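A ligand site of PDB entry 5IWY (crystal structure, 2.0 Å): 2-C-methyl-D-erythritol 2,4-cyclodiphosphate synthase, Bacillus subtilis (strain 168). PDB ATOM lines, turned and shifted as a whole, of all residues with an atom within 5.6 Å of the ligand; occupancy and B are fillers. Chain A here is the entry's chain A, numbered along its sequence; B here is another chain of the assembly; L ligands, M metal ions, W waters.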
ATOM      1  N   ILE A  99     -22.042 -24.455   5.347  1.00  0.00           N
ATOM      2  CA  ILE A  99     -22.670 -23.574   4.399  1.00  0.00           C
ATOM      3  C   ILE A  99     -23.925 -23.026   5.080  1.00  0.00           C
ATOM      4  O   ILE A  99     -24.749 -23.784   5.551  1.00  0.00           O
ATOM      5  CB  ILE A  99     -23.062 -24.349   3.110  1.00  0.00           C
ATOM      6  CG1 ILE A  99     -21.832 -25.059   2.502  1.00  0.00           C
ATOM      7  CG2 ILE A  99     -23.711 -23.416   2.111  1.00  0.00           C
ATOM      8  CD1 ILE A  99     -22.133 -26.047   1.372  1.00  0.00           C
ATOM      9  N   ALA A 101     -27.108 -21.216   4.065  1.00  0.00           N
ATOM     10  CA  ALA A 101     -27.899 -20.857   2.885  1.00  0.00           C
ATOM     11  C   ALA A 101     -29.348 -21.293   3.063  1.00  0.00           C
ATOM     12  O   ALA A 101     -29.574 -22.429   3.505  1.00  0.00           O
ATOM     13  CB  ALA A 101     -27.324 -21.537   1.672  1.00  0.00           C
ATOM     14  N   GLN A 102     -30.296 -20.429   2.682  1.00  0.00           N
ATOM     15  CA  GLN A 102     -31.699 -20.812   2.742  1.00  0.00           C
ATOM     16  C   GLN A 102     -31.984 -21.818   1.642  1.00  0.00           C
ATOM     17  O   GLN A 102     -32.645 -22.835   1.867  1.00  0.00           O
ATOM     18  CB  GLN A 102     -32.629 -19.596   2.628  1.00  0.00           C
ATOM     19  CG  GLN A 102     -34.070 -19.914   3.011  1.00  0.00           C
ATOM     20  CD  GLN A 102     -34.214 -20.319   4.472  1.00  0.00           C
ATOM     21  OE1 GLN A 102     -33.628 -19.715   5.393  1.00  0.00           O
ATOM     22  NE2 GLN A 102     -35.001 -21.358   4.688  1.00  0.00           N
ATOM     23  N   LYS A 103     -31.445 -21.535   0.457  1.00  0.00           N
ATOM     24  CA  LYS A 103     -31.486 -22.433  -0.702  1.00  0.00           C
ATOM     25  C   LYS A 103     -30.287 -22.178  -1.672  1.00  0.00           C
ATOM     26  O   LYS A 103     -29.646 -21.121  -1.623  1.00  0.00           O
ATOM     27  CB  LYS A 103     -32.848 -22.283  -1.424  1.00  0.00           C
ATOM     28  CG  LYS A 103     -33.399 -20.859  -1.453  1.00  0.00           C
ATOM     29  CD  LYS A 103     -34.833 -20.793  -1.972  1.00  0.00           C
ATOM     30  CE  LYS A 103     -35.336 -19.360  -1.909  1.00  0.00           C
ATOM     31  NZ  LYS A 103     -36.560 -19.143  -2.724  1.00  0.00           N
ATOM     32  N   PRO A 104     -29.947 -23.150  -2.525  1.00  0.00           N
ATOM     33  CA  PRO A 104     -30.599 -24.473  -2.627  1.00  0.00           C
ATOM     34  C   PRO A 104     -30.202 -25.446  -1.544  1.00  0.00           C
ATOM     35  O   PRO A 104     -29.353 -25.144  -0.699  1.00  0.00           O
ATOM     36  CB  PRO A 104     -30.095 -24.999  -3.972  1.00  0.00           C
ATOM     37  CG  PRO A 104     -28.808 -24.284  -4.205  1.00  0.00           C
ATOM     38  CD  PRO A 104     -29.037 -22.900  -3.651  1.00  0.00           C
ATOM     39  N   LYS A 105     -30.889 -26.574  -1.555  1.00  0.00           N
ATOM     40  CA  LYS A 105     -30.565 -27.738  -0.740  1.00  0.00           C
ATOM     41  C   LYS A 105     -29.162 -28.212  -1.128  1.00  0.00           C
ATOM     42  O   LYS A 105     -28.901 -28.467  -2.289  1.00  0.00           O
ATOM     43  CB  LYS A 105     -31.598 -28.855  -1.013  1.00  0.00           C
ATOM     44  CG  LYS A 105     -31.455 -30.091  -0.160  1.00  0.00           C
ATOM     45  CD  LYS A 105     -31.935 -29.858   1.259  1.00  0.00           C
ATOM     46  CE  LYS A 105     -31.818 -31.120   2.108  1.00  0.00           C
ATOM     47  NZ  LYS A 105     -32.145 -30.830   3.542  1.00  0.00           N
ATOM     48  N   MET A 106     -28.255 -28.233  -0.173  1.00  0.00           N
ATOM     49  CA  MET A 106     -26.860 -28.519  -0.456  1.00  0.00           C
ATOM     50  C   MET A 106     -26.557 -30.006  -0.456  1.00  0.00           C
ATOM     51  O   MET A 106     -25.724 -30.458  -1.226  1.00  0.00           O
ATOM     52  CB  MET A 106     -25.945 -27.805   0.561  1.00  0.00           C
ATOM     53  CG  MET A 106     -25.995 -26.304   0.441  1.00  0.00           C
ATOM     54  SD  MET A 106     -25.342 -25.699  -1.116  1.00  0.00           S
ATOM     55  CE  MET A 106     -26.198 -24.153  -1.185  1.00  0.00           C
ATOM     56  N   LEU A 107     -27.262 -30.716   0.427  1.00  0.00           N
ATOM     57  CA  LEU A 107     -27.136 -32.148   0.681  1.00  0.00           C
ATOM     58  C   LEU A 107     -26.698 -33.087  -0.457  1.00  0.00           C
ATOM     59  O   LEU A 107     -25.800 -33.894  -0.252  1.00  0.00           O
ATOM     60  CB  LEU A 107     -28.460 -32.660   1.273  1.00  0.00           C
ATOM     61  CG  LEU A 107     -28.570 -34.168   1.513  1.00  0.00           C
ATOM     62  CD1 LEU A 107     -27.776 -34.519   2.763  1.00  0.00           C
ATOM     63  CD2 LEU A 107     -30.030 -34.579   1.610  1.00  0.00           C
ATOM     64  N   PRO A 108     -27.357 -33.002  -1.641  1.00  0.00           N
ATOM     65  CA  PRO A 108     -26.905 -33.879  -2.732  1.00  0.00           C
ATOM     66  C   PRO A 108     -25.485 -33.629  -3.244  1.00  0.00           C
ATOM     67  O   PRO A 108     -24.882 -34.532  -3.813  1.00  0.00           O
ATOM     68  CB  PRO A 108     -27.932 -33.630  -3.849  1.00  0.00           C
ATOM     69  CG  PRO A 108     -28.764 -32.467  -3.414  1.00  0.00           C
ATOM     70  CD  PRO A 108     -28.693 -32.437  -1.918  1.00  0.00           C
ATOM     71  N   ALA A 132     -24.535 -28.149   6.010  1.00  0.00           N
ATOM     72  CA  ALA A 132     -25.349 -26.968   5.636  1.00  0.00           C
ATOM     73  C   ALA A 132     -26.421 -26.709   6.674  1.00  0.00           C
ATOM     74  O   ALA A 132     -26.826 -27.647   7.370  1.00  0.00           O
ATOM     75  CB  ALA A 132     -25.945 -27.190   4.275  1.00  0.00           C
ATOM     76  N   THR A 133     -26.785 -25.434   6.892  1.00  0.00           N
ATOM     77  CA  THR A 133     -27.939 -25.064   7.752  1.00  0.00           C
ATOM     78  C   THR A 133     -28.561 -23.823   7.099  1.00  0.00           C
ATOM     79  O   THR A 133     -27.912 -23.107   6.357  1.00  0.00           O
ATOM     80  CB  THR A 133     -27.589 -24.811   9.263  1.00  0.00           C
ATOM     81  OG1 THR A 133     -28.786 -24.608  10.064  1.00  0.00           O
ATOM     82  CG2 THR A 133     -26.665 -23.593   9.457  1.00  0.00           C
ATOM     83  N   THR A 134     -29.850 -23.641   7.302  1.00  0.00           N
ATOM     84  CA  THR A 134     -30.549 -22.411   6.901  1.00  0.00           C
ATOM     85  C   THR A 134     -30.515 -21.570   8.163  1.00  0.00           C
ATOM     86  O   THR A 134     -30.046 -22.026   9.218  1.00  0.00           O
ATOM     87  CB  THR A 134     -32.013 -22.678   6.504  1.00  0.00           C
ATOM     88  OG1 THR A 134     -32.746 -23.082   7.659  1.00  0.00           O
ATOM     89  CG2 THR A 134     -32.135 -23.793   5.486  1.00  0.00           C
ATOM     90  N   THR A 135     -31.026 -20.365   8.066  1.00  0.00           N
ATOM     91  CA  THR A 135     -31.249 -19.513   9.235  1.00  0.00           C
ATOM     92  C   THR A 135     -32.761 -19.314   9.463  1.00  0.00           C
ATOM     93  O   THR A 135     -33.206 -18.271   9.979  1.00  0.00           O
ATOM     94  CB  THR A 135     -30.505 -18.164   9.038  1.00  0.00           C
ATOM     95  OG1 THR A 135     -30.978 -17.533   7.862  1.00  0.00           O
ATOM     96  CG2 THR A 135     -29.000 -18.401   8.925  1.00  0.00           C
ATOM     97  N   GLU A 136     -33.548 -20.296   9.023  1.00  0.00           N
ATOM     98  CA  GLU A 136     -34.989 -20.365   9.262  1.00  0.00           C
ATOM     99  C   GLU A 136     -35.643 -19.091   8.809  1.00  0.00           C
ATOM    100  O   GLU A 136     -36.390 -18.475   9.570  1.00  0.00           O
ATOM    101  CB  GLU A 136     -35.247 -20.614  10.748  1.00  0.00           C
ATOM    102  CG  GLU A 136     -34.643 -21.903  11.275  1.00  0.00           C
ATOM    103  CD  GLU A 136     -35.282 -23.154  10.660  1.00  0.00           C
ATOM    104  OE1 GLU A 136     -36.431 -23.084  10.116  1.00  0.00           O
ATOM    105  OE2 GLU A 136     -34.601 -24.201  10.711  1.00  0.00           O
ATOM    106  N   ASP B   9     -26.192 -22.904  14.603  1.00  0.00           N
ATOM    107  CA  ASP B   9     -27.654 -23.149  14.378  1.00  0.00           C
ATOM    108  C   ASP B   9     -28.409 -21.880  14.726  1.00  0.00           C
ATOM    109  O   ASP B   9     -27.914 -21.031  15.479  1.00  0.00           O
ATOM    110  CB  ASP B   9     -28.124 -24.345  15.209  1.00  0.00           C
ATOM    111  CG  ASP B   9     -29.436 -24.965  14.709  1.00  0.00           C
ATOM    112  OD1 ASP B   9     -29.812 -24.800  13.538  1.00  0.00           O
ATOM    113  OD2 ASP B   9     -30.140 -25.604  15.531  1.00  0.00           O
ATOM    114  N   ASP B  47     -23.992 -30.874  16.209  1.00  0.00           N
ATOM    115  CA  ASP B  47     -23.332 -30.552  14.931  1.00  0.00           C
ATOM    116  C   ASP B  47     -21.779 -30.469  15.008  1.00  0.00           C
ATOM    117  O   ASP B  47     -21.104 -31.040  14.159  1.00  0.00           O
ATOM    118  CB  ASP B  47     -23.942 -29.290  14.263  1.00  0.00           C
ATOM    119  CG  ASP B  47     -24.928 -29.616  13.124  1.00  0.00           C
ATOM    120  OD1 ASP B  47     -25.308 -30.795  12.969  1.00  0.00           O
ATOM    121  OD2 ASP B  47     -25.274 -28.709  12.330  1.00  0.00           O
ATOM    122  N   ASP B  57     -24.047 -33.900   9.483  1.00  0.00           N
ATOM    123  CA  ASP B  57     -24.784 -33.033  10.385  1.00  0.00           C
ATOM    124  C   ASP B  57     -26.081 -33.671  10.911  1.00  0.00           C
ATOM    125  O   ASP B  57     -26.448 -34.779  10.501  1.00  0.00           O
ATOM    126  CB  ASP B  57     -25.036 -31.666   9.703  1.00  0.00           C
ATOM    127  CG  ASP B  57     -25.897 -31.759   8.412  1.00  0.00           C
ATOM    128  OD1 ASP B  57     -26.766 -32.653   8.254  1.00  0.00           O
ATOM    129  OD2 ASP B  57     -25.727 -30.888   7.514  1.00  0.00           O
ATOM    130  N   ILE B  58     -26.724 -33.012  11.875  1.00  0.00           N
ATOM    131  CA  ILE B  58     -27.924 -33.548  12.504  1.00  0.00           C
ATOM    132  C   ILE B  58     -29.009 -33.888  11.471  1.00  0.00           C
ATOM    133  O   ILE B  58     -29.625 -34.925  11.593  1.00  0.00           O
ATOM    134  CB  ILE B  58     -28.462 -32.656  13.643  1.00  0.00           C
ATOM    135  CG1 ILE B  58     -28.800 -31.245  13.136  1.00  0.00           C
ATOM    136  CG2 ILE B  58     -27.511 -32.714  14.841  1.00  0.00           C
ATOM    137  CD1 ILE B  58     -28.603 -30.106  14.126  1.00  0.00           C
ATOM    138  N   GLY B  59     -29.177 -33.068  10.432  1.00  0.00           N
ATOM    139  CA  GLY B  59     -30.106 -33.348   9.337  1.00  0.00           C
ATOM    140  C   GLY B  59     -29.890 -34.673   8.625  1.00  0.00           C
ATOM    141  O   GLY B  59     -30.876 -35.337   8.227  1.00  0.00           O
ATOM    142  N   LYS B  60     -28.632 -35.084   8.474  1.00  0.00           N
ATOM    143  CA  LYS B  60     -28.356 -36.391   7.906  1.00  0.00           C
ATOM    144  C   LYS B  60     -28.813 -37.507   8.863  1.00  0.00           C
ATOM    145  O   LYS B  60     -29.273 -38.533   8.402  1.00  0.00           O
ATOM    146  CB  LYS B  60     -26.864 -36.552   7.525  1.00  0.00           C
ATOM    147  CG  LYS B  60     -26.462 -37.977   7.132  1.00  0.00           C
ATOM    148  CD  LYS B  60     -25.285 -38.049   6.176  1.00  0.00           C
ATOM    149  CE  LYS B  60     -23.938 -37.948   6.880  1.00  0.00           C
ATOM    150  NZ  LYS B  60     -23.472 -39.231   7.486  1.00  0.00           N
ATOM    151  N   ASP B  64     -35.939 -33.886   9.156  1.00  0.00           N
ATOM    152  CA  ASP B  64     -37.290 -33.355   9.463  1.00  0.00           C
ATOM    153  C   ASP B  64     -38.376 -34.225   8.918  1.00  0.00           C
ATOM    154  O   ASP B  64     -39.363 -34.504   9.599  1.00  0.00           O
ATOM    155  CB  ASP B  64     -37.492 -31.991   8.817  1.00  0.00           C
ATOM    156  CG  ASP B  64     -36.490 -30.990   9.265  1.00  0.00           C
ATOM    157  OD1 ASP B  64     -36.323 -30.849  10.495  1.00  0.00           O
ATOM    158  OD2 ASP B  64     -35.838 -30.368   8.404  1.00  0.00           O
HETATM  159  O1  LIG L   1     -33.514 -26.309   8.218  1.00  0.00           O
HETATM  160  P1  LIG L   1     -32.146 -26.470   8.874  1.00  0.00           P
HETATM  161  O2  LIG L   1     -32.076 -27.166  10.179  1.00  0.00           O
HETATM  162  O3  LIG L   1     -31.300 -25.235   8.908  1.00  0.00           O
HETATM  163  O4  LIG L   1     -31.458 -27.509   7.875  1.00  0.00           O
HETATM  164  C1  LIG L   1     -31.996 -28.824   7.752  1.00  0.00           C
HETATM  165  C2  LIG L   1     -30.969 -29.809   7.253  1.00  0.00           C
HETATM  166  O5  LIG L   1     -30.930 -29.673   5.838  1.00  0.00           O
HETATM  167  C3  LIG L   1     -29.522 -29.614   7.792  1.00  0.00           C
HETATM  168  O6  LIG L   1     -29.222 -30.328   9.007  1.00  0.00           O
HETATM  169  C4  LIG L   1     -28.733 -30.093   6.604  1.00  0.00           C
HETATM  170  O7  LIG L   1     -28.654 -31.495   6.781  1.00  0.00           O
HETATM  171  C5  LIG L   1     -29.564 -29.748   5.358  1.00  0.00           C
HETATM  172  N1  LIG L   1     -29.399 -28.462   4.619  1.00  0.00           N
HETATM  173  C6  LIG L   1     -29.058 -28.471   3.263  1.00  0.00           C
HETATM  174  N2  LIG L   1     -28.983 -27.307   2.535  1.00  0.00           N
HETATM  175  C7  LIG L   1     -29.224 -26.107   3.099  1.00  0.00           C
HETATM  176  C8  LIG L   1     -29.579 -26.061   4.429  1.00  0.00           C
HETATM  177  C9  LIG L   1     -29.682 -27.265   5.173  1.00  0.00           C
HETATM  178  O8  LIG L   1     -28.802 -29.557   2.672  1.00  0.00           O
HETATM  179  N3  LIG L   1     -29.122 -24.974   2.348  1.00  0.00           N
HETATM  180 MG    MG M   1     -31.629 -26.733  15.164  1.00  0.00          MG
HETATM  181  O   HOH W   1     -33.737 -27.727  11.854  1.00  0.00           O
HETATM  182  O   HOH W   2     -25.775 -30.685   5.086  1.00  0.00           O
HETATM  183  O   HOH W   3     -31.421 -29.662  11.337  1.00  0.00           O
HETATM  184  O   HOH W   4     -27.223 -29.016  10.117  1.00  0.00           O
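The side-chain carboxylate of Glu 136 lies close to an oxygen (O1) of the ligand, 3.4 Å away.
Ala 132 touches the ligand.
Lys 60 of chain B touches the ligand (N to O7, 3.97 Å).
Hydrophobic or aromatic side chains that line the ligand: Ala 101, Met 106, Leu 107 and Ala 132.
12 residues have an atom within 4 Å of the ligand: Ala 101, Pro 104, Lys 105, Met 106, Leu 107, Ala 132, Thr 133, Thr 134, Glu 136, Asp 57 of chain B, Gly 59 of chain B and Lys 60 of chain B.
OD1 of Asp 57 of chain B lies within hydrogen-bond range of O7 of the ligand, at 2.7 Å.
O3 of the ligand is in hydrogen-bond range of N of Thr 134.
An oxygen (O3) of the ligand is in hydrogen-bond range of the side-chain hydroxyl (OG1) of Thr 134, 2.9 Å away.
The backbone carbonyl oxygen of Ala 101 lies within hydrogen-bond range of a nitrogen (N3) of the ligand (2.8 Å).
The side-chain hydroxyl (OG1) of Thr 133 lies within hydrogen-bond range of an oxygen (O3) of the ligand (2.8 Å).
The side-chain amino group of Lys 105 is in hydrogen-bond range of an oxygen (O5) of the ligand, at 2.8 Å.
The backbone NH (N) of Met 106 is in hydrogen-bond range of a nitrogen (N2) of the ligand.
N of Leu 107 is in hydrogen-bond range of O8 of the ligand, 3.0 Å away.
N3 of the ligand sits at hydrogen-bond distance from O of Pro 104, at 3.1 Å.
N of Gly 59 of chain B lies within hydrogen-bond range of O6 of the ligand (3.1 Å).
Water W4 lies within hydrogen-bond range of an oxygen (O6) of the ligand (2.6 Å), the side-chain carboxylate (OD2) of Asp 47 of chain B (3.0 Å) and the backbone carbonyl oxygen (O) of Ala 132 (3.1 Å).
Water W2 lies within hydrogen-bond range of OD2 of Asp 57 of chain B (2.4 Å), N of Ala 132 (3.0 Å) and O7 of the ligand (3.4 Å).
The side-chain carboxylate (OD1) of Asp 57 of chain B sits close to the backbone NH (N) of Gly 59 of chain B (3.3 Å).
The side-chain carboxylate of Asp 57 of chain B lies within hydrogen-bond range of the backbone NH of Ala 132.
N of Lys 60 of chain B lies within hydrogen-bond range of OD1 of Asp 57 of chain B, at 3.1 Å.
The backbone NH (N) of Glu 136 is in hydrogen-bond range of the side-chain hydroxyl (OG1) of Thr 134, 3.2 Å away.
N of Ala 101 sits at hydrogen-bond distance from O of Thr 133, at 3.1 Å.
The backbone NH (N) of Thr 133 sits at hydrogen-bond distance from the backbone carbonyl oxygen (O) of Ile 99.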
